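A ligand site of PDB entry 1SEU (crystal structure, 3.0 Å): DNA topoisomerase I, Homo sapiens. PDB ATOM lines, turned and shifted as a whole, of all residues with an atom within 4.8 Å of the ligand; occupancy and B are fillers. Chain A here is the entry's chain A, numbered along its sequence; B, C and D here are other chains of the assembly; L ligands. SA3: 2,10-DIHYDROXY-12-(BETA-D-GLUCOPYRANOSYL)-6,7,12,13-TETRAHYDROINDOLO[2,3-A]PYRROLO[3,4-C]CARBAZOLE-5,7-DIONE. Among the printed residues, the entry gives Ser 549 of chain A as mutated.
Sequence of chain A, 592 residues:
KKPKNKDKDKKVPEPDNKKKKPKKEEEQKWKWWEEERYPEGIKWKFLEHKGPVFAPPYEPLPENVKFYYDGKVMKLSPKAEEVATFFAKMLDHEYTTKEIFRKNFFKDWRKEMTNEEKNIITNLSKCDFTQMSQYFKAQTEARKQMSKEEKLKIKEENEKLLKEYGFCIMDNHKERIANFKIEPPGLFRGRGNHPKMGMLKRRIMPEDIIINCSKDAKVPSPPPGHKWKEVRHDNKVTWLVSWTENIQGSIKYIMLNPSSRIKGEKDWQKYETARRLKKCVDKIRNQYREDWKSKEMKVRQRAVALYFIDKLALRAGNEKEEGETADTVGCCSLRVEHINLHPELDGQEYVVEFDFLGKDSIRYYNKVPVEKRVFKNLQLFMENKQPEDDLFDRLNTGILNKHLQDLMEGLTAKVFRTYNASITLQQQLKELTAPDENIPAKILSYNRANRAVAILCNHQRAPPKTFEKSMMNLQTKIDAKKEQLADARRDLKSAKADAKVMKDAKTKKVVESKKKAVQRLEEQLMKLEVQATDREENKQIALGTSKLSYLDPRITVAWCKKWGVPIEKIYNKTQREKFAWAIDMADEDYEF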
ATOM      1  N   ALA A 178      14.369  27.213  -2.385  1.00  0.00           N
ATOM      2  CA  ALA A 178      14.153  26.655  -1.059  1.00  0.00           C
ATOM      3  C   ALA A 178      15.304  25.810  -0.504  1.00  0.00           C
ATOM      4  O   ALA A 178      15.882  26.159   0.527  1.00  0.00           O
ATOM      5  CB  ALA A 178      12.870  25.839  -1.026  1.00  0.00           C
ATOM      6  N   ASN A 179      15.656  24.736  -1.205  1.00  0.00           N
ATOM      7  CA  ASN A 179      16.696  23.824  -0.733  1.00  0.00           C
ATOM      8  C   ASN A 179      17.627  23.343  -1.839  1.00  0.00           C
ATOM      9  O   ASN A 179      17.731  22.132  -2.089  1.00  0.00           O
ATOM     10  CB  ASN A 179      16.010  22.621  -0.042  1.00  0.00           C
ATOM     11  CG  ASN A 179      14.997  21.876  -0.965  1.00  0.00           C
ATOM     12  OD1 ASN A 179      14.363  22.472  -1.848  1.00  0.00           O
ATOM     13  ND2 ASN A 179      14.893  20.554  -0.789  1.00  0.00           N
ATOM     14  N   GLU A 183      20.063  16.292  -0.155  1.00  0.00           N
ATOM     15  CA  GLU A 183      20.206  15.510   1.073  1.00  0.00           C
ATOM     16  C   GLU A 183      21.393  14.522   1.080  1.00  0.00           C
ATOM     17  O   GLU A 183      21.558  13.730   0.145  1.00  0.00           O
ATOM     18  CB  GLU A 183      18.885  14.786   1.380  1.00  0.00           C
ATOM     19  CG  GLU A 183      17.809  14.881   0.270  1.00  0.00           C
ATOM     20  CD  GLU A 183      16.423  15.277   0.790  1.00  0.00           C
ATOM     21  OE1 GLU A 183      15.680  14.382   1.284  1.00  0.00           O
ATOM     22  OE2 GLU A 183      16.043  16.470   0.697  1.00  0.00           O
ATOM     23  N   ARG A 191       9.690   8.999  11.780  1.00  0.00           N
ATOM     24  CA  ARG A 191       9.043   9.301  13.041  1.00  0.00           C
ATOM     25  C   ARG A 191       8.174   8.168  13.549  1.00  0.00           C
ATOM     26  O   ARG A 191       7.415   7.539  12.792  1.00  0.00           O
ATOM     27  CB  ARG A 191       8.247  10.614  12.963  1.00  0.00           C
ATOM     28  CG  ARG A 191       9.103  11.854  13.235  1.00  0.00           C
ATOM     29  CD  ARG A 191       8.355  13.154  12.996  1.00  0.00           C
ATOM     30  NE  ARG A 191       8.054  13.402  11.587  1.00  0.00           N
ATOM     31  CZ  ARG A 191       8.571  14.385  10.855  1.00  0.00           C
ATOM     32  NH1 ARG A 191       9.437  15.253  11.389  1.00  0.00           N
ATOM     33  NH2 ARG A 191       8.170  14.557   9.600  1.00  0.00           N
ATOM     34  N   LYS A 252      11.089  13.508  -4.385  1.00  0.00           N
ATOM     35  CA  LYS A 252      11.601  14.633  -3.579  1.00  0.00           C
ATOM     36  C   LYS A 252      11.828  15.809  -4.536  1.00  0.00           C
ATOM     37  O   LYS A 252      12.202  15.588  -5.685  1.00  0.00           O
ATOM     38  CB  LYS A 252      12.916  14.229  -2.928  1.00  0.00           C
ATOM     39  CG  LYS A 252      13.003  14.362  -1.432  1.00  0.00           C
ATOM     40  CD  LYS A 252      12.124  13.366  -0.682  1.00  0.00           C
ATOM     41  CE  LYS A 252      12.484  13.369   0.810  1.00  0.00           C
ATOM     42  NZ  LYS A 252      11.689  12.424   1.664  1.00  0.00           N
ATOM     43  N   TYR A 253      11.588  17.047  -4.077  1.00  0.00           N
ATOM     44  CA  TYR A 253      11.712  18.241  -4.958  1.00  0.00           C
ATOM     45  C   TYR A 253      12.489  19.454  -4.447  1.00  0.00           C
ATOM     46  O   TYR A 253      12.629  19.678  -3.251  1.00  0.00           O
ATOM     47  CB  TYR A 253      10.309  18.758  -5.307  1.00  0.00           C
ATOM     48  CG  TYR A 253       9.329  17.771  -5.909  1.00  0.00           C
ATOM     49  CD1 TYR A 253       8.410  17.079  -5.096  1.00  0.00           C
ATOM     50  CD2 TYR A 253       9.280  17.547  -7.298  1.00  0.00           C
ATOM     51  CE1 TYR A 253       7.472  16.182  -5.670  1.00  0.00           C
ATOM     52  CE2 TYR A 253       8.355  16.661  -7.876  1.00  0.00           C
ATOM     53  CZ  TYR A 253       7.455  15.977  -7.056  1.00  0.00           C
ATOM     54  OH  TYR A 253       6.546  15.108  -7.615  1.00  0.00           O
ATOM     55  N   MET A 255      12.037  23.180  -4.626  1.00  0.00           N
ATOM     56  CA  MET A 255      11.039  24.201  -4.895  1.00  0.00           C
ATOM     57  C   MET A 255      11.589  25.589  -4.619  1.00  0.00           C
ATOM     58  O   MET A 255      12.719  25.750  -4.161  1.00  0.00           O
ATOM     59  CB  MET A 255       9.796  23.953  -4.014  1.00  0.00           C
ATOM     60  CG  MET A 255       9.375  22.475  -3.883  1.00  0.00           C
ATOM     61  SD  MET A 255       7.622  22.128  -4.117  1.00  0.00           S
ATOM     62  CE  MET A 255       7.614  21.570  -5.831  1.00  0.00           C
ATOM     63  N   LEU A 548       2.469  29.644  10.575  1.00  0.00           N
ATOM     64  CA  LEU A 548       2.854  29.648   9.175  1.00  0.00           C
ATOM     65  C   LEU A 548       1.845  29.044   8.206  1.00  0.00           C
ATOM     66  O   LEU A 548       1.571  29.641   7.143  1.00  0.00           O
ATOM     67  CB  LEU A 548       4.203  28.942   8.970  1.00  0.00           C
ATOM     68  CG  LEU A 548       5.525  29.678   9.225  1.00  0.00           C
ATOM     69  CD1 LEU A 548       5.713  29.879  10.717  1.00  0.00           C
ATOM     70  CD2 LEU A 548       6.681  28.866   8.647  1.00  0.00           C
ATOM     71  N   SER A 549       1.270  27.907   8.582  1.00  0.00           N
ATOM     72  CA  SER A 549       0.390  27.212   7.673  1.00  0.00           C
ATOM     73  C   SER A 549      -1.125  27.221   7.875  1.00  0.00           C
ATOM     74  O   SER A 549      -1.841  26.711   7.010  1.00  0.00           O
ATOM     75  CB  SER A 549       0.901  25.773   7.525  1.00  0.00           C
ATOM     76  OG  SER A 549       2.252  25.773   7.095  1.00  0.00           O
ATOM     77  S5' TGP B   1       5.978  25.357   9.627  1.00  0.00           S
ATOM     78  N9  TGP B   1       9.217  22.917   9.886  1.00  0.00           N
ATOM     79  C4  TGP B   1      10.204  22.031   9.523  1.00  0.00           C
ATOM     80  N3  TGP B   1      10.454  20.862  10.126  1.00  0.00           N
ATOM     81  C2  TGP B   1      11.436  20.205   9.524  1.00  0.00           C
ATOM     82  N2  TGP B   1      11.782  18.980   9.962  1.00  0.00           N
ATOM     83  N1  TGP B   1      12.129  20.691   8.438  1.00  0.00           N
ATOM     84  C6  TGP B   1      11.885  21.904   7.807  1.00  0.00           C
ATOM     85  O6  TGP B   1      12.568  22.253   6.847  1.00  0.00           O
ATOM     86  C5  TGP B   1      10.828  22.597   8.430  1.00  0.00           C
ATOM     87  N7  TGP B   1      10.237  23.812   8.108  1.00  0.00           N
ATOM     88  C8  TGP B   1       9.298  23.962   8.997  1.00  0.00           C
ATOM     89  C2' TGP B   1       8.031  24.035  11.759  1.00  0.00           C
ATOM     90  C5' TGP B   1       5.115  23.847  10.118  1.00  0.00           C
ATOM     91  C4' TGP B   1       5.952  23.054  11.100  1.00  0.00           C
ATOM     92  O4' TGP B   1       7.032  22.403  10.405  1.00  0.00           O
ATOM     93  C1' TGP B   1       8.275  22.761  10.975  1.00  0.00           C
ATOM     94  C3' TGP B   1       6.587  23.868  12.223  1.00  0.00           C
ATOM     95  O3' TGP B   1       6.568  23.127  13.434  1.00  0.00           O
ATOM     96  P    DC C  12      20.552  14.433   9.240  1.00  0.00           P
ATOM     97  OP1  DC C  12      21.351  13.622  10.208  1.00  0.00           O
ATOM     98  OP2  DC C  12      20.711  14.211   7.774  1.00  0.00           O
ATOM     99  O5'  DC C  12      19.027  14.266   9.602  1.00  0.00           O
ATOM    100  C5'  DC C  12      18.115  13.842   8.616  1.00  0.00           C
ATOM    101  C4'  DC C  12      16.740  13.693   9.212  1.00  0.00           C
ATOM    102  O4'  DC C  12      16.135  15.002   9.379  1.00  0.00           O
ATOM    103  C3'  DC C  12      15.847  12.946   8.230  1.00  0.00           C
ATOM    104  O3'  DC C  12      15.004  12.032   8.910  1.00  0.00           O
ATOM    105  C2'  DC C  12      15.063  14.025   7.529  1.00  0.00           C
ATOM    106  C1'  DC C  12      14.954  15.096   8.588  1.00  0.00           C
ATOM    107  N1   DC C  12      14.890  16.452   8.024  1.00  0.00           N
ATOM    108  C2   DC C  12      13.924  17.339   8.527  1.00  0.00           C
ATOM    109  O2   DC C  12      13.212  16.982   9.503  1.00  0.00           O
ATOM    110  N3   DC C  12      13.771  18.552   7.941  1.00  0.00           N
ATOM    111  C4   DC C  12      14.548  18.892   6.922  1.00  0.00           C
ATOM    112  N4   DC C  12      14.322  20.075   6.331  1.00  0.00           N
ATOM    113  C5   DC C  12      15.585  18.035   6.441  1.00  0.00           C
ATOM    114  C6   DC C  12      15.719  16.843   7.009  1.00  0.00           C
ATOM    115  P    DA C  13      14.644  10.650   8.203  1.00  0.00           P
ATOM    116  OP1  DA C  13      14.964   9.558   9.172  1.00  0.00           O
ATOM    117  OP2  DA C  13      15.271  10.661   6.850  1.00  0.00           O
ATOM    118  O5'  DA C  13      13.083  10.761   8.009  1.00  0.00           O
ATOM    119  C5'  DA C  13      12.518  11.923   7.454  1.00  0.00           C
ATOM    120  C4'  DA C  13      11.108  12.062   7.945  1.00  0.00           C
ATOM    121  O4'  DA C  13      10.554  13.332   7.511  1.00  0.00           O
ATOM    122  C3'  DA C  13      10.170  10.978   7.421  1.00  0.00           C
ATOM    123  O3'  DA C  13       9.366  10.495   8.509  1.00  0.00           O
ATOM    124  C2'  DA C  13       9.374  11.684   6.333  1.00  0.00           C
ATOM    125  C1'  DA C  13       9.339  13.119   6.838  1.00  0.00           C
ATOM    126  N9   DA C  13       9.222  14.140   5.812  1.00  0.00           N
ATOM    127  C8   DA C  13       9.979  14.285   4.691  1.00  0.00           C
ATOM    128  N7   DA C  13       9.665  15.325   3.969  1.00  0.00           N
ATOM    129  C5   DA C  13       8.610  15.902   4.674  1.00  0.00           C
ATOM    130  C6   DA C  13       7.825  17.029   4.426  1.00  0.00           C
ATOM    131  N6   DA C  13       7.993  17.815   3.362  1.00  0.00           N
ATOM    132  N1   DA C  13       6.862  17.333   5.314  1.00  0.00           N
ATOM    133  C2   DA C  13       6.697  16.540   6.366  1.00  0.00           C
ATOM    134  N3   DA C  13       7.366  15.449   6.703  1.00  0.00           N
ATOM    135  C4   DA C  13       8.327  15.183   5.798  1.00  0.00           C
ATOM    136  P    DT D   9       1.517  24.404  -2.242  1.00  0.00           P
ATOM    137  OP1  DT D   9       0.138  24.953  -1.987  1.00  0.00           O
ATOM    138  OP2  DT D   9       2.657  25.307  -2.555  1.00  0.00           O
ATOM    139  O5'  DT D   9       1.958  23.505  -1.005  1.00  0.00           O
ATOM    140  C5'  DT D   9       1.699  23.934   0.309  1.00  0.00           C
ATOM    141  C4'  DT D   9       0.552  23.151   0.894  1.00  0.00           C
ATOM    142  O4'  DT D   9       0.775  21.740   0.693  1.00  0.00           O
ATOM    143  C3'  DT D   9       0.525  23.362   2.394  1.00  0.00           C
ATOM    144  O3'  DT D   9      -0.786  23.469   2.934  1.00  0.00           O
ATOM    145  C2'  DT D   9       1.311  22.187   2.953  1.00  0.00           C
ATOM    146  C1'  DT D   9       1.232  21.112   1.890  1.00  0.00           C
ATOM    147  N1   DT D   9       2.552  20.515   1.602  1.00  0.00           N
ATOM    148  C2   DT D   9       2.900  19.303   2.202  1.00  0.00           C
ATOM    149  O2   DT D   9       2.212  18.734   3.037  1.00  0.00           O
ATOM    150  N3   DT D   9       4.103  18.799   1.796  1.00  0.00           N
ATOM    151  C4   DT D   9       4.996  19.378   0.914  1.00  0.00           C
ATOM    152  O4   DT D   9       6.038  18.789   0.612  1.00  0.00           O
ATOM    153  C5   DT D   9       4.605  20.657   0.389  1.00  0.00           C
ATOM    154  C7   DT D   9       5.549  21.413  -0.483  1.00  0.00           C
ATOM    155  C6   DT D   9       3.409  21.148   0.737  1.00  0.00           C
ATOM    156  P    DT D  10      -0.951  24.145   4.367  1.00  0.00           P
ATOM    157  OP1  DT D  10      -2.397  24.201   4.690  1.00  0.00           O
ATOM    158  OP2  DT D  10      -0.145  25.385   4.365  1.00  0.00           O
ATOM    159  O5'  DT D  10      -0.268  23.087   5.348  1.00  0.00           O
ATOM    160  C5'  DT D  10      -0.907  21.850   5.595  1.00  0.00           C
ATOM    161  C4'  DT D  10      -0.189  21.100   6.695  1.00  0.00           C
ATOM    162  O4'  DT D  10       0.960  20.388   6.197  1.00  0.00           O
ATOM    163  C3'  DT D  10       0.296  21.956   7.853  1.00  0.00           C
ATOM    164  C2'  DT D  10       1.789  22.082   7.586  1.00  0.00           C
ATOM    165  C1'  DT D  10       2.096  20.722   6.964  1.00  0.00           C
ATOM    166  N1   DT D  10       3.245  20.645   6.065  1.00  0.00           N
ATOM    167  C2   DT D  10       4.108  19.583   6.186  1.00  0.00           C
ATOM    168  O2   DT D  10       4.002  18.738   7.071  1.00  0.00           O
ATOM    169  N3   DT D  10       5.088  19.520   5.251  1.00  0.00           N
ATOM    170  C4   DT D  10       5.309  20.406   4.229  1.00  0.00           C
ATOM    171  O4   DT D  10       6.208  20.218   3.441  1.00  0.00           O
ATOM    172  C5   DT D  10       4.413  21.525   4.184  1.00  0.00           C
ATOM    173  C7   DT D  10       4.613  22.566   3.127  1.00  0.00           C
ATOM    174  C6   DT D  10       3.441  21.594   5.091  1.00  0.00           C
HETATM  175  O1  SA3 L   1      13.983  16.050   4.257  1.00  0.00           O
HETATM  176  C6  SA3 L   1      13.186  16.629   4.650  1.00  0.00           C
HETATM  177  C5  SA3 L   1      12.569  16.148   5.775  1.00  0.00           C
HETATM  178  C4  SA3 L   1      11.508  16.866   6.365  1.00  0.00           C
HETATM  179  C3  SA3 L   1      11.060  18.081   5.835  1.00  0.00           C
HETATM  180  C2  SA3 L   1      11.678  18.670   4.616  1.00  0.00           C
HETATM  181  N9  SA3 L   1      10.956  19.896   4.387  1.00  0.00           N
HETATM  182  C1  SA3 L   1      12.757  17.901   4.054  1.00  0.00           C
HETATM  183  C11 SA3 L   1      10.013  18.889   6.319  1.00  0.00           C
HETATM  184  C15 SA3 L   1       9.096  18.806   7.418  1.00  0.00           C
HETATM  185  C18 SA3 L   1       8.938  17.805   8.467  1.00  0.00           C
HETATM  186  O37 SA3 L   1       9.576  16.791   8.638  1.00  0.00           O
HETATM  187  N17 SA3 L   1       7.926  18.218   9.242  1.00  0.00           N
HETATM  188  C14 SA3 L   1       8.116  19.817   7.636  1.00  0.00           C
HETATM  189  C16 SA3 L   1       7.378  19.396   8.834  1.00  0.00           C
HETATM  190  O38 SA3 L   1       6.431  19.988   9.383  1.00  0.00           O
HETATM  191  C13 SA3 L   1       8.026  20.962   6.767  1.00  0.00           C
HETATM  192  C21 SA3 L   1       7.226  22.153   6.637  1.00  0.00           C
HETATM  193  C20 SA3 L   1       7.701  22.929   5.466  1.00  0.00           C
HETATM  194  N19 SA3 L   1       8.711  22.192   4.954  1.00  0.00           N
HETATM  195  C12 SA3 L   1       8.934  21.046   5.673  1.00  0.00           C
HETATM  196  C10 SA3 L   1       9.963  19.995   5.415  1.00  0.00           C
HETATM  197  C25 SA3 L   1       6.158  22.650   7.390  1.00  0.00           C
HETATM  198  C24 SA3 L   1       5.553  23.881   7.004  1.00  0.00           C
HETATM  199  C23 SA3 L   1       6.022  24.641   5.867  1.00  0.00           C
HETATM  200  C22 SA3 L   1       7.129  24.143   5.081  1.00  0.00           C
HETATM  201  O2  SA3 L   1       5.528  25.597   5.602  1.00  0.00           O
HETATM  202  C31 SA3 L   1      11.026  20.951   3.371  1.00  0.00           C
HETATM  203  C32 SA3 L   1      12.111  21.919   2.843  1.00  0.00           C
HETATM  204  O32 SA3 L   1      11.687  23.265   3.009  1.00  0.00           O
HETATM  205  C33 SA3 L   1      12.287  21.469   1.398  1.00  0.00           C
HETATM  206  O33 SA3 L   1      12.594  20.100   1.613  1.00  0.00           O
HETATM  207  C34 SA3 L   1      10.977  21.546   0.530  1.00  0.00           C
HETATM  208  O34 SA3 L   1      10.640  22.877   0.248  1.00  0.00           O
HETATM  209  C35 SA3 L   1       9.788  20.869   1.268  1.00  0.00           C
HETATM  210  C36 SA3 L   1       9.743  19.329   1.084  1.00  0.00           C
HETATM  211  O36 SA3 L   1       9.680  19.013  -0.309  1.00  0.00           O
HETATM  212  O5  SA3 L   1       9.834  21.199   2.650  1.00  0.00           O
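An oxygen (O33) of the ligand is in hydrogen-bond range of the side-chain amide nitrogen (ND2) of Asn 179 (3.4 Å). NH2 of Arg 191 lies within hydrogen-bond range of O37 of the ligand (2.8 Å). O38 of the ligand lies close to O4' of TGP 1 of chain B (2.7 Å).
O2 of DC 12 of chain C lies close to N2 of TGP 1 of chain B. ND2 of Asn 179 lies within hydrogen-bond range of O of Tyr 253, at 3.5 Å. NH2 of Arg 191 sits at hydrogen-bond distance from N3 of DA 13 of chain C, 3.1 Å away. The backbone NH of Ala 178 sits at hydrogen-bond distance from the backbone carbonyl oxygen of Met 255 (2.8 Å).
O37 of the ligand sits close to N3 of DA 13 of chain C (3.2 Å). Merely in contact with the ligand: Ala 178 (3.9 Å), Glu 183 (3.8 Å), Ser 549 (3.6 Å), DC 12 of chain C (3.2 Å), DT 9 of chain D (3.8 Å) and DT 10 of chain D (3.5 Å). Hydrophobic or aromatic side chains that line the ligand: Ala 178. The nearest printed residue that does not touch the ligand is Tyr 253 (4.2 Å).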
